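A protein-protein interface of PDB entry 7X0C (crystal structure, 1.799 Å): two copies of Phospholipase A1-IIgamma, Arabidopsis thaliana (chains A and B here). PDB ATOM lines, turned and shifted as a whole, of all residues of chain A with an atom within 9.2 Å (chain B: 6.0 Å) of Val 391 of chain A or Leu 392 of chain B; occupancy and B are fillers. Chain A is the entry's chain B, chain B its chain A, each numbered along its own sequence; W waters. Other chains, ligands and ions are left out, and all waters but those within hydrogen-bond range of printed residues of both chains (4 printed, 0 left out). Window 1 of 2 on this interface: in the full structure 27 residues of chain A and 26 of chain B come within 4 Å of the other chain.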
ATOM      1  N   TYR A  59     -35.468   5.212  24.504  1.00  0.00           N
ATOM      2  CA  TYR A  59     -34.433   6.100  23.969  1.00  0.00           C
ATOM      3  C   TYR A  59     -33.073   5.413  23.955  1.00  0.00           C
ATOM      4  O   TYR A  59     -32.254   5.656  23.046  1.00  0.00           O
ATOM      5  CB  TYR A  59     -34.346   7.392  24.796  1.00  0.00           C
ATOM      6  CG  TYR A  59     -35.573   8.300  24.723  1.00  0.00           C
ATOM      7  CD1 TYR A  59     -36.201   8.539  23.494  1.00  0.00           C
ATOM      8  CD2 TYR A  59     -36.073   8.926  25.856  1.00  0.00           C
ATOM      9  CE1 TYR A  59     -37.301   9.422  23.401  1.00  0.00           C
ATOM     10  CE2 TYR A  59     -37.185   9.806  25.783  1.00  0.00           C
ATOM     11  CZ  TYR A  59     -37.788  10.036  24.547  1.00  0.00           C
ATOM     12  OH  TYR A  59     -38.869  10.881  24.460  1.00  0.00           O
ATOM     13  N   ASP A  60     -32.795   4.585  24.949  1.00  0.00           N
ATOM     14  CA  ASP A  60     -31.443   4.060  25.057  1.00  0.00           C
ATOM     15  C   ASP A  60     -31.177   2.952  24.037  1.00  0.00           C
ATOM     16  O   ASP A  60     -30.009   2.713  23.696  1.00  0.00           O
ATOM     17  CB  ASP A  60     -31.166   3.590  26.492  1.00  0.00           C
ATOM     18  CG  ASP A  60     -31.146   4.756  27.492  1.00  0.00           C
ATOM     19  OD1 ASP A  60     -31.058   5.932  27.070  1.00  0.00           O
ATOM     20  OD2 ASP A  60     -31.261   4.519  28.709  1.00  0.00           O
ATOM     21  N   PHE A  62     -32.870   3.168  20.891  1.00  0.00           N
ATOM     22  CA  PHE A  62     -33.293   3.655  19.589  1.00  0.00           C
ATOM     23  C   PHE A  62     -32.095   4.236  18.825  1.00  0.00           C
ATOM     24  O   PHE A  62     -31.416   5.144  19.307  1.00  0.00           O
ATOM     25  CB  PHE A  62     -34.392   4.688  19.791  1.00  0.00           C
ATOM     26  CG  PHE A  62     -34.967   5.194  18.508  1.00  0.00           C
ATOM     27  CD1 PHE A  62     -35.633   4.335  17.645  1.00  0.00           C
ATOM     28  CD2 PHE A  62     -34.878   6.546  18.187  1.00  0.00           C
ATOM     29  CE1 PHE A  62     -36.197   4.831  16.447  1.00  0.00           C
ATOM     30  CE2 PHE A  62     -35.449   7.034  16.986  1.00  0.00           C
ATOM     31  CZ  PHE A  62     -36.066   6.154  16.131  1.00  0.00           C
ATOM     32  N   ASN A  63     -31.833   3.717  17.632  1.00  0.00           N
ATOM     33  CA  ASN A  63     -30.659   4.126  16.862  1.00  0.00           C
ATOM     34  C   ASN A  63     -30.938   5.452  16.167  1.00  0.00           C
ATOM     35  O   ASN A  63     -31.831   5.519  15.317  1.00  0.00           O
ATOM     36  CB  ASN A  63     -30.346   3.029  15.841  1.00  0.00           C
ATOM     37  CG  ASN A  63     -29.054   3.270  15.090  1.00  0.00           C
ATOM     38  OD1 ASN A  63     -28.565   4.392  15.024  1.00  0.00           O
ATOM     39  ND2 ASN A  63     -28.504   2.209  14.518  1.00  0.00           N
ATOM     40  N   ILE A  64     -30.201   6.509  16.525  1.00  0.00           N
ATOM     41  CA  ILE A  64     -30.489   7.847  16.001  1.00  0.00           C
ATOM     42  C   ILE A  64     -29.406   8.313  15.041  1.00  0.00           C
ATOM     43  O   ILE A  64     -29.381   9.487  14.662  1.00  0.00           O
ATOM     44  CB  ILE A  64     -30.688   8.881  17.120  1.00  0.00           C
ATOM     45  CG1 ILE A  64     -29.429   9.028  17.966  1.00  0.00           C
ATOM     46  CG2 ILE A  64     -31.914   8.532  17.990  1.00  0.00           C
ATOM     47  CD1 ILE A  64     -29.537  10.142  19.030  1.00  0.00           C
ATOM     48  N   ASN A  65     -28.536   7.414  14.597  1.00  0.00           N
ATOM     49  CA  ASN A  65     -27.406   7.791  13.729  1.00  0.00           C
ATOM     50  C   ASN A  65     -27.838   7.671  12.272  1.00  0.00           C
ATOM     51  O   ASN A  65     -27.847   6.573  11.707  1.00  0.00           O
ATOM     52  CB  ASN A  65     -26.211   6.903  14.046  1.00  0.00           C
ATOM     53  CG  ASN A  65     -24.986   7.246  13.221  1.00  0.00           C
ATOM     54  OD1 ASN A  65     -25.018   8.163  12.399  1.00  0.00           O
ATOM     55  ND2 ASN A  65     -23.902   6.507  13.441  1.00  0.00           N
ATOM     56  N   ILE A  75     -31.232  -0.869  18.724  1.00  0.00           N
ATOM     57  CA  ILE A  75     -29.856  -1.386  18.861  1.00  0.00           C
ATOM     58  C   ILE A  75     -29.870  -2.789  19.454  1.00  0.00           C
ATOM     59  O   ILE A  75     -29.220  -3.710  18.934  1.00  0.00           O
ATOM     60  CB  ILE A  75     -29.028  -0.424  19.732  1.00  0.00           C
ATOM     61  CG1 ILE A  75     -28.889   0.936  19.006  1.00  0.00           C
ATOM     62  CG2 ILE A  75     -27.647  -1.040  20.115  1.00  0.00           C
ATOM     63  CD1 ILE A  75     -28.407   2.048  19.874  1.00  0.00           C
ATOM     64  N   TYR A  76     -30.571  -2.965  20.585  1.00  0.00           N
ATOM     65  CA  TYR A  76     -30.543  -4.210  21.337  1.00  0.00           C
ATOM     66  C   TYR A  76     -31.707  -5.110  20.943  1.00  0.00           C
ATOM     67  O   TYR A  76     -32.790  -4.639  20.587  1.00  0.00           O
ATOM     68  CB  TYR A  76     -30.574  -3.938  22.857  1.00  0.00           C
ATOM     69  CG  TYR A  76     -29.374  -3.066  23.263  1.00  0.00           C
ATOM     70  CD1 TYR A  76     -28.060  -3.576  23.162  1.00  0.00           C
ATOM     71  CD2 TYR A  76     -29.539  -1.734  23.640  1.00  0.00           C
ATOM     72  CE1 TYR A  76     -26.950  -2.788  23.488  1.00  0.00           C
ATOM     73  CE2 TYR A  76     -28.443  -0.934  23.962  1.00  0.00           C
ATOM     74  CZ  TYR A  76     -27.156  -1.474  23.895  1.00  0.00           C
ATOM     75  OH  TYR A  76     -26.082  -0.698  24.221  1.00  0.00           O
ATOM     76  N   ASN A 373     -27.403  13.647  31.740  1.00  0.00           N
ATOM     77  CA  ASN A 373     -26.652  14.092  30.567  1.00  0.00           C
ATOM     78  C   ASN A 373     -26.606  13.074  29.427  1.00  0.00           C
ATOM     79  O   ASN A 373     -25.782  13.233  28.513  1.00  0.00           O
ATOM     80  CB  ASN A 373     -25.235  14.489  30.999  1.00  0.00           C
ATOM     81  CG  ASN A 373     -25.148  15.963  31.422  1.00  0.00           C
ATOM     82  OD1 ASN A 373     -26.174  16.628  31.594  1.00  0.00           O
ATOM     83  ND2 ASN A 373     -23.913  16.482  31.569  1.00  0.00           N
ATOM     84  N   LYS A 374     -27.452  12.032  29.452  1.00  0.00           N
ATOM     85  CA  LYS A 374     -27.440  11.068  28.339  1.00  0.00           C
ATOM     86  C   LYS A 374     -27.558  11.763  26.978  1.00  0.00           C
ATOM     87  O   LYS A 374     -26.830  11.438  26.021  1.00  0.00           O
ATOM     88  CB  LYS A 374     -28.563  10.041  28.516  1.00  0.00           C
ATOM     89  CG  LYS A 374     -28.224   8.911  29.490  1.00  0.00           C
ATOM     90  CD  LYS A 374     -29.383   7.944  29.584  1.00  0.00           C
ATOM     91  CE  LYS A 374     -29.055   6.800  30.498  1.00  0.00           C
ATOM     92  NZ  LYS A 374     -30.308   6.010  30.757  1.00  0.00           N
ATOM     93  N   SER A 375     -28.477  12.709  26.847  1.00  0.00           N
ATOM     94  CA  SER A 375     -28.671  13.281  25.523  1.00  0.00           C
ATOM     95  C   SER A 375     -28.722  14.798  25.529  1.00  0.00           C
ATOM     96  O   SER A 375     -29.050  15.386  24.497  1.00  0.00           O
ATOM     97  CB  SER A 375     -29.924  12.691  24.859  1.00  0.00           C
ATOM     98  OG  SER A 375     -31.080  12.867  25.652  1.00  0.00           O
ATOM     99  N   GLY A 387     -21.361  16.200  28.700  1.00  0.00           N
ATOM    100  CA  GLY A 387     -22.693  16.370  28.132  1.00  0.00           C
ATOM    101  C   GLY A 387     -22.939  15.381  27.009  1.00  0.00           C
ATOM    102  O   GLY A 387     -22.006  14.895  26.377  1.00  0.00           O
ATOM    103  N   LYS A 388     -24.224  15.062  26.780  1.00  0.00           N
ATOM    104  CA  LYS A 388     -24.662  14.168  25.704  1.00  0.00           C
ATOM    105  C   LYS A 388     -23.777  12.928  25.585  1.00  0.00           C
ATOM    106  O   LYS A 388     -23.181  12.645  24.538  1.00  0.00           O
ATOM    107  CB  LYS A 388     -24.716  14.915  24.357  1.00  0.00           C
ATOM    108  CG  LYS A 388     -25.464  16.229  24.403  1.00  0.00           C
ATOM    109  CD  LYS A 388     -25.512  16.893  23.009  1.00  0.00           C
ATOM    110  CE  LYS A 388     -26.394  18.141  23.039  1.00  0.00           C
ATOM    111  NZ  LYS A 388     -26.531  18.761  21.677  1.00  0.00           N
ATOM    112  N   TRP A 389     -23.697  12.168  26.667  1.00  0.00           N
ATOM    113  CA  TRP A 389     -22.699  11.111  26.691  1.00  0.00           C
ATOM    114  C   TRP A 389     -23.157   9.769  26.128  1.00  0.00           C
ATOM    115  O   TRP A 389     -22.297   8.931  25.853  1.00  0.00           O
ATOM    116  CB  TRP A 389     -22.150  10.905  28.101  1.00  0.00           C
ATOM    117  CG  TRP A 389     -23.078  10.663  29.270  1.00  0.00           C
ATOM    118  CD1 TRP A 389     -23.404  11.560  30.252  1.00  0.00           C
ATOM    119  CD2 TRP A 389     -23.756   9.432  29.605  1.00  0.00           C
ATOM    120  NE1 TRP A 389     -24.236  10.956  31.189  1.00  0.00           N
ATOM    121  CE2 TRP A 389     -24.462   9.654  30.821  1.00  0.00           C
ATOM    122  CE3 TRP A 389     -23.823   8.166  29.005  1.00  0.00           C
ATOM    123  CZ2 TRP A 389     -25.208   8.643  31.455  1.00  0.00           C
ATOM    124  CZ3 TRP A 389     -24.580   7.174  29.620  1.00  0.00           C
ATOM    125  CH2 TRP A 389     -25.261   7.418  30.840  1.00  0.00           C
ATOM    126  N   ARG A 390     -24.453   9.518  25.932  1.00  0.00           N
ATOM    127  CA  ARG A 390     -24.857   8.175  25.505  1.00  0.00           C
ATOM    128  C   ARG A 390     -24.437   7.892  24.053  1.00  0.00           C
ATOM    129  O   ARG A 390     -24.823   8.615  23.129  1.00  0.00           O
ATOM    130  CB  ARG A 390     -26.373   7.977  25.652  1.00  0.00           C
ATOM    131  CG  ARG A 390     -26.845   6.574  25.200  1.00  0.00           C
ATOM    132  CD  ARG A 390     -28.400   6.462  25.109  1.00  0.00           C
ATOM    133  NE  ARG A 390     -28.874   7.463  24.162  1.00  0.00           N
ATOM    134  CZ  ARG A 390     -29.955   8.226  24.308  1.00  0.00           C
ATOM    135  NH1 ARG A 390     -30.752   8.074  25.377  1.00  0.00           N
ATOM    136  NH2 ARG A 390     -30.250   9.153  23.367  1.00  0.00           N
ATOM    137  N   VAL A 391     -23.686   6.820  23.858  1.00  0.00           N
ATOM    138  CA  VAL A 391     -23.188   6.438  22.531  1.00  0.00           C
ATOM    139  C   VAL A 391     -22.601   5.033  22.622  1.00  0.00           C
ATOM    140  O   VAL A 391     -22.013   4.652  23.645  1.00  0.00           O
ATOM    141  CB  VAL A 391     -22.149   7.461  22.004  1.00  0.00           C
ATOM    142  CG1 VAL A 391     -20.888   7.436  22.852  1.00  0.00           C
ATOM    143  CG2 VAL A 391     -21.786   7.206  20.511  1.00  0.00           C
ATOM    144  N   LEU A 392     -22.810   4.214  21.594  1.00  0.00           N
ATOM    145  CA  LEU A 392     -22.136   2.919  21.572  1.00  0.00           C
ATOM    146  C   LEU A 392     -20.640   3.140  21.476  1.00  0.00           C
ATOM    147  O   LEU A 392     -20.185   4.135  20.917  1.00  0.00           O
ATOM    148  CB  LEU A 392     -22.565   2.107  20.349  1.00  0.00           C
ATOM    149  CG  LEU A 392     -23.977   1.567  20.336  1.00  0.00           C
ATOM    150  CD1 LEU A 392     -24.318   1.040  18.899  1.00  0.00           C
ATOM    151  CD2 LEU A 392     -24.153   0.460  21.401  1.00  0.00           C
ATOM    152  N   LYS A 393     -19.870   2.169  21.939  1.00  0.00           N
ATOM    153  CA  LYS A 393     -18.431   2.269  21.708  1.00  0.00           C
ATOM    154  C   LYS A 393     -18.144   2.393  20.217  1.00  0.00           C
ATOM    155  O   LYS A 393     -18.660   1.617  19.402  1.00  0.00           O
ATOM    156  CB  LYS A 393     -17.719   1.053  22.280  1.00  0.00           C
ATOM    157  CG  LYS A 393     -16.186   1.149  22.045  1.00  0.00           C
ATOM    158  CD  LYS A 393     -15.458  -0.071  22.631  1.00  0.00           C
ATOM    159  CE  LYS A 393     -13.954   0.018  22.295  1.00  0.00           C
ATOM    160  NZ  LYS A 393     -13.144  -1.081  22.942  1.00  0.00           N
ATOM    161  N   ASN A 394     -17.361   3.404  19.850  1.00  0.00           N
ATOM    162  CA  ASN A 394     -16.945   3.583  18.460  1.00  0.00           C
ATOM    163  C   ASN A 394     -18.133   3.768  17.525  1.00  0.00           C
ATOM    164  O   ASN A 394     -18.049   3.460  16.327  1.00  0.00           O
ATOM    165  CB  ASN A 394     -16.050   2.418  18.011  1.00  0.00           C
ATOM    166  CG  ASN A 394     -14.668   2.525  18.624  1.00  0.00           C
ATOM    167  OD1 ASN A 394     -14.228   3.618  18.950  1.00  0.00           O
ATOM    168  ND2 ASN A 394     -13.984   1.398  18.793  1.00  0.00           N
ATOM    169  N   LYS A 395     -19.224   4.334  18.072  1.00  0.00           N
ATOM    170  CA  LYS A 395     -20.499   4.474  17.380  1.00  0.00           C
ATOM    171  C   LYS A 395     -20.991   3.154  16.797  1.00  0.00           C
ATOM    172  O   LYS A 395     -21.787   3.148  15.856  1.00  0.00           O
ATOM    173  CB  LYS A 395     -20.409   5.534  16.275  1.00  0.00           C
ATOM    174  CG  LYS A 395     -20.068   6.941  16.782  1.00  0.00           C
ATOM    175  CD  LYS A 395     -20.148   7.975  15.681  1.00  0.00           C
ATOM    176  CE  LYS A 395     -19.745   9.357  16.196  1.00  0.00           C
ATOM    177  NZ  LYS A 395     -19.807  10.275  15.052  1.00  0.00           N
ATOM    178  N   GLY A 396     -20.562   2.033  17.349  1.00  0.00           N
ATOM    179  CA  GLY A 396     -20.933   0.732  16.829  1.00  0.00           C
ATOM    180  C   GLY A 396     -19.923   0.090  15.892  1.00  0.00           C
ATOM    181  O   GLY A 396     -20.043  -1.112  15.620  1.00  0.00           O
ATOM    182  N   MET A 397     -18.946   0.839  15.378  1.00  0.00           N
ATOM    183  CA  MET A 397     -17.899   0.191  14.578  1.00  0.00           C
ATOM    184  C   MET A 397     -17.175  -0.862  15.415  1.00  0.00           C
ATOM    185  O   MET A 397     -16.832  -0.634  16.584  1.00  0.00           O
ATOM    186  CB  MET A 397     -16.897   1.236  14.051  1.00  0.00           C
ATOM    187  CG  MET A 397     -17.500   2.246  13.061  1.00  0.00           C
ATOM    188  SD  MET A 397     -18.020   1.436  11.497  1.00  0.00           S
ATOM    189  CE  MET A 397     -16.375   0.868  10.911  1.00  0.00           C
ATOM    190  N   ASP A 409     -24.181  -1.977  14.902  1.00  0.00           N
ATOM    191  CA  ASP A 409     -25.008  -1.180  15.801  1.00  0.00           C
ATOM    192  C   ASP A 409     -26.412  -1.748  15.918  1.00  0.00           C
ATOM    193  O   ASP A 409     -27.320  -1.048  16.379  1.00  0.00           O
ATOM    194  CB  ASP A 409     -25.040   0.280  15.349  1.00  0.00           C
ATOM    195  CG  ASP A 409     -25.568   0.470  13.920  1.00  0.00           C
ATOM    196  OD1 ASP A 409     -25.837  -0.519  13.182  1.00  0.00           O
ATOM    197  OD2 ASP A 409     -25.717   1.639  13.543  1.00  0.00           O
ATOM    198  N   ILE B  75      -6.053   6.720  28.065  1.00  0.00           N
ATOM    199  CA  ILE B  75      -7.237   5.952  28.476  1.00  0.00           C
ATOM    200  C   ILE B  75      -6.829   4.568  28.981  1.00  0.00           C
ATOM    201  O   ILE B  75      -7.249   4.124  30.057  1.00  0.00           O
ATOM    202  CB  ILE B  75      -8.195   5.824  27.279  1.00  0.00           C
ATOM    203  CG1 ILE B  75      -8.724   7.204  26.882  1.00  0.00           C
ATOM    204  CG2 ILE B  75      -9.334   4.756  27.562  1.00  0.00           C
ATOM    205  CD1 ILE B  75      -9.424   7.230  25.537  1.00  0.00           C
ATOM    206  N   TYR B  76      -6.014   3.859  28.199  1.00  0.00           N
ATOM    207  CA  TYR B  76      -5.636   2.487  28.515  1.00  0.00           C
ATOM    208  C   TYR B  76      -4.323   2.413  29.292  1.00  0.00           C
ATOM    209  O   TYR B  76      -3.427   3.251  29.141  1.00  0.00           O
ATOM    210  CB  TYR B  76      -5.529   1.649  27.234  1.00  0.00           C
ATOM    211  CG  TYR B  76      -6.875   1.651  26.495  1.00  0.00           C
ATOM    212  CD1 TYR B  76      -8.000   1.007  27.065  1.00  0.00           C
ATOM    213  CD2 TYR B  76      -7.034   2.323  25.292  1.00  0.00           C
ATOM    214  CE1 TYR B  76      -9.247   1.021  26.400  1.00  0.00           C
ATOM    215  CE2 TYR B  76      -8.263   2.352  24.630  1.00  0.00           C
ATOM    216  CZ  TYR B  76      -9.365   1.696  25.197  1.00  0.00           C
ATOM    217  OH  TYR B  76     -10.589   1.733  24.557  1.00  0.00           O
ATOM    218  N   ARG B 390     -14.518   7.247  16.496  1.00  0.00           N
ATOM    219  CA  ARG B 390     -13.788   6.735  17.656  1.00  0.00           C
ATOM    220  C   ARG B 390     -14.275   7.407  18.946  1.00  0.00           C
ATOM    221  O   ARG B 390     -14.193   8.633  19.081  1.00  0.00           O
ATOM    222  CB  ARG B 390     -12.283   6.959  17.518  1.00  0.00           C
ATOM    223  CG  ARG B 390     -11.505   6.361  18.725  1.00  0.00           C
ATOM    224  CD  ARG B 390      -9.995   6.753  18.696  1.00  0.00           C
ATOM    225  NE  ARG B 390      -9.868   8.205  18.674  1.00  0.00           N
ATOM    226  CZ  ARG B 390      -9.001   8.870  17.919  1.00  0.00           C
ATOM    227  NH1 ARG B 390      -8.142   8.201  17.137  1.00  0.00           N
ATOM    228  NH2 ARG B 390      -9.004  10.215  17.934  1.00  0.00           N
ATOM    229  N   VAL B 391     -14.743   6.602  19.896  1.00  0.00           N
ATOM    230  CA  VAL B 391     -15.246   7.105  21.180  1.00  0.00           C
ATOM    231  C   VAL B 391     -15.440   5.913  22.124  1.00  0.00           C
ATOM    232  O   VAL B 391     -15.753   4.788  21.693  1.00  0.00           O
ATOM    233  CB  VAL B 391     -16.555   7.901  20.997  1.00  0.00           C
ATOM    234  CG1 VAL B 391     -17.705   6.981  20.480  1.00  0.00           C
ATOM    235  CG2 VAL B 391     -16.987   8.563  22.331  1.00  0.00           C
ATOM    236  N   LEU B 392     -15.187   6.115  23.409  1.00  0.00           N
ATOM    237  CA  LEU B 392     -15.521   5.070  24.371  1.00  0.00           C
ATOM    238  C   LEU B 392     -17.032   4.911  24.455  1.00  0.00           C
ATOM    239  O   LEU B 392     -17.781   5.863  24.228  1.00  0.00           O
ATOM    240  CB  LEU B 392     -15.002   5.428  25.768  1.00  0.00           C
ATOM    241  CG  LEU B 392     -13.486   5.411  25.980  1.00  0.00           C
ATOM    242  CD1 LEU B 392     -13.170   6.143  27.323  1.00  0.00           C
ATOM    243  CD2 LEU B 392     -12.937   3.970  25.940  1.00  0.00           C
ATOM    244  N   LYS B 393     -17.476   3.722  24.849  1.00  0.00           N
ATOM    245  CA  LYS B 393     -18.908   3.554  25.104  1.00  0.00           C
ATOM    246  C   LYS B 393     -19.370   4.591  26.125  1.00  0.00           C
ATOM    247  O   LYS B 393     -18.736   4.758  27.172  1.00  0.00           O
ATOM    248  CB  LYS B 393     -19.196   2.153  25.619  1.00  0.00           C
ATOM    249  CG  LYS B 393     -20.728   1.933  25.863  1.00  0.00           C
ATOM    250  CD  LYS B 393     -21.046   0.499  26.297  1.00  0.00           C
ATOM    251  CE  LYS B 393     -22.559   0.362  26.590  1.00  0.00           C
ATOM    252  NZ  LYS B 393     -22.965  -1.027  26.991  1.00  0.00           N
ATOM    253  N   ASN B 394     -20.444   5.321  25.806  1.00  0.00           N
ATOM    254  CA  ASN B 394     -21.006   6.308  26.730  1.00  0.00           C
ATOM    255  C   ASN B 394     -19.982   7.361  27.140  1.00  0.00           C
ATOM    256  O   ASN B 394     -20.098   7.984  28.211  1.00  0.00           O
ATOM    257  CB  ASN B 394     -21.614   5.597  27.954  1.00  0.00           C
ATOM    258  CG  ASN B 394     -22.875   4.830  27.566  1.00  0.00           C
ATOM    259  OD1 ASN B 394     -23.541   5.236  26.631  1.00  0.00           O
ATOM    260  ND2 ASN B 394     -23.215   3.743  28.295  1.00  0.00           N
ATOM    261  N   LYS B 395     -18.996   7.610  26.261  1.00  0.00           N
ATOM    262  CA  LYS B 395     -17.896   8.530  26.559  1.00  0.00           C
ATOM    263  C   LYS B 395     -17.137   8.138  27.827  1.00  0.00           C
ATOM    264  O   LYS B 395     -16.412   8.958  28.404  1.00  0.00           O
ATOM    265  CB  LYS B 395     -18.381   9.976  26.664  1.00  0.00           C
ATOM    266  CG  LYS B 395     -18.996  10.544  25.370  1.00  0.00           C
ATOM    267  CD  LYS B 395     -19.294  12.024  25.475  1.00  0.00           C
ATOM    268  CE  LYS B 395     -19.949  12.568  24.204  1.00  0.00           C
ATOM    269  NZ  LYS B 395     -20.222  14.032  24.423  1.00  0.00           N
ATOM    270  N   GLY B 396     -17.257   6.876  28.234  1.00  0.00           N
ATOM    271  CA  GLY B 396     -16.614   6.363  29.423  1.00  0.00           C
ATOM    272  C   GLY B 396     -17.485   6.352  30.673  1.00  0.00           C
ATOM    273  O   GLY B 396     -17.083   5.737  31.665  1.00  0.00           O
ATOM    274  N   VAL B 408     -15.551   6.709  33.884  1.00  0.00           N
ATOM    275  CA  VAL B 408     -14.463   5.747  34.000  1.00  0.00           C
ATOM    276  C   VAL B 408     -13.768   5.697  32.647  1.00  0.00           C
ATOM    277  O   VAL B 408     -14.000   4.785  31.836  1.00  0.00           O
ATOM    278  CB  VAL B 408     -14.972   4.367  34.446  1.00  0.00           C
ATOM    279  CG1 VAL B 408     -13.799   3.415  34.684  1.00  0.00           C
ATOM    280  CG2 VAL B 408     -15.806   4.511  35.721  1.00  0.00           C
ATOM    281  N   ASP B 409     -12.983   6.733  32.365  1.00  0.00           N
ATOM    282  CA  ASP B 409     -12.319   6.883  31.074  1.00  0.00           C
ATOM    283  C   ASP B 409     -10.808   6.783  31.209  1.00  0.00           C
ATOM    284  O   ASP B 409     -10.074   7.222  30.311  1.00  0.00           O
ATOM    285  CB  ASP B 409     -12.712   8.199  30.406  1.00  0.00           C
ATOM    286  CG  ASP B 409     -12.363   9.444  31.249  1.00  0.00           C
ATOM    287  OD1 ASP B 409     -11.896   9.313  32.420  1.00  0.00           O
ATOM    288  OD2 ASP B 409     -12.582  10.560  30.736  1.00  0.00           O
ATOM    289  N   HIS B 410     -10.330   6.201  32.311  1.00  0.00           N
ATOM    290  CA  HIS B 410      -8.892   6.110  32.582  1.00  0.00           C
ATOM    291  C   HIS B 410      -8.620   4.853  33.394  1.00  0.00           C
ATOM    292  O   HIS B 410      -9.106   4.722  34.524  1.00  0.00           O
ATOM    293  CB  HIS B 410      -8.407   7.372  33.322  1.00  0.00           C
ATOM    294  CG  HIS B 410      -7.008   7.263  33.838  1.00  0.00           C
ATOM    295  ND1 HIS B 410      -5.901   7.397  33.018  1.00  0.00           N
ATOM    296  CD2 HIS B 410      -6.531   7.015  35.083  1.00  0.00           C
ATOM    297  CE1 HIS B 410      -4.803   7.267  33.747  1.00  0.00           C
ATOM    298  NE2 HIS B 410      -5.155   7.039  34.999  1.00  0.00           N
HETATM  299  O   HOH W   1     -23.465  -1.680  24.030  1.00  0.00           O
HETATM  300  O   HOH W   2     -10.451   0.584  21.909  1.00  0.00           O
HETATM  301  O   HOH W   3     -12.808   0.624  25.524  1.00  0.00           O
HETATM  302  O   HOH W   4     -26.036   0.238  26.953  1.00  0.00           O
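The backbone NH of Asn 394 of chain A is in hydrogen-bond range of the backbone carbonyl oxygen of Val 391 of chain B (2.8 Å). The backbone carbonyl oxygen of Trp 389 of chain A sits close to the backbone carbonyl oxygen of Asn 394 of chain B, at 3.4 Å. N of Asn 394 of chain B sits at hydrogen-bond distance from O of Val 391 of chain A (2.8 Å). The side-chain amino group of Lys 395 of chain B lies within hydrogen-bond range of the backbone carbonyl oxygen of Gly 387 of chain A. NZ of Lys 395 of chain B lies close to O of Lys 388 of chain A (3.3 Å).
O of Asn 373 of chain A is in hydrogen-bond range of N of Trp 389 of chain A (3.0 Å). The backbone NH (N) of Lys 388 of chain A is in hydrogen-bond range of the backbone carbonyl oxygen (O) of Asn 373 of chain A (3.0 Å). NH1 of Arg 390 of chain A lies within salt-bridge range of OD1 of Asp 60 of chain A (2.7 Å). The backbone carbonyl oxygen (O) of Lys 374 of chain A sits at hydrogen-bond distance from the backbone NH (N) of Arg 390 of chain A (3.1 Å).
Trp 389 of chain A touches Lys 395 of chain B. CA of Arg 390 of chain A touches OD1 of Asn 394 of chain B, 3.4 Å away. Val 391 of chain A touches Leu 392 of chain B. Lys 393 of chain B touches Val 391 of chain A. Leu 392 of chain A touches Val 391 of chain B (O to CG1, 3.8 Å). CA of Lys 393 of chain A touches O of Val 391 of chain B, at 3.7 Å. CA of Lys 393 of chain B touches N of Lys 393 of chain A, at 3.6 Å.
Printed residues of chain B within 4 Å of Val 391 of chain A: Val 391 (3.996 Å), Leu 392 (3.7 Å), Lys 393 (3.6 Å), Asn 394 (2.8 Å) and Lys 395 (3.9 Å). Of chain A, only Val 391 comes within 4 Å of Leu 392 of chain B. Asn 394 of chain B touches just these residues of chain A: Trp 389, Arg 390 and Val 391. Printed residues of chain A within 4 Å of Lys 393 of chain B: Val 391 (3.6 Å) and Lys 393 (3.6 Å). Of the printed residues of chain B, Lys 395 of chain A touches Val 391 (3.9 Å). Gly 396 of chain A touches none of the printed residues of chain B. The nearest printed residue of chain B that does not touch Val 391 of chain A is Gly 396 of chain B (6.5 Å).
Of the 12 printed residues of chain B, 6 touch a printed residue of chain A. Printed residues of chain B that touch a printed residue of chain A: Arg 390, Val 391, Leu 392, Lys 393, Asn 394 and Lys 395. Printed residues of chain A that touch a printed residue of chain B: Gly 387, Lys 388, Trp 389, Arg 390, Val 391, Leu 392, Lys 393, Asn 394 and Lys 395. Along chain A the printed residues that touch a printed residue of chain B span positions 387 to 395. Among the printed residues, no Asp or Glu carboxylate lies within 4 Å of a Lys or Arg side-chain nitrogen of the other chain.
Val 391 of chain B touches its own counterpart, Val 391 of chain A. Val 391 of chain A touches Lys 393 of chain B, and with the chains exchanged Lys 393 of chain A touches Val 391 of chain B. Val 391 of chain A touches Asn 394 of chain B, and with the chains exchanged Asn 394 of chain A touches Val 391 of chain B. Lys 393 of chain A touches its own counterpart, Lys 393 of chain B.
Water W3 bridges OH of Tyr 76 of chain B (2.7 Å) and NZ of Lys 393 of chain A (3.1 Å). Water W1 bridges the side-chain hydroxyl of Tyr 76 of chain A (2.8 Å) and the side-chain amino group of Lys 393 of chain B (3.1 Å). Water W4 lies within hydrogen-bond range of OH of Tyr 76 of chain A and NZ of Lys 393 of chain B. Water W2 lies within hydrogen-bond range of the side-chain hydroxyl of Tyr 76 of chain B and the side-chain amino group of Lys 393 of chain A.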
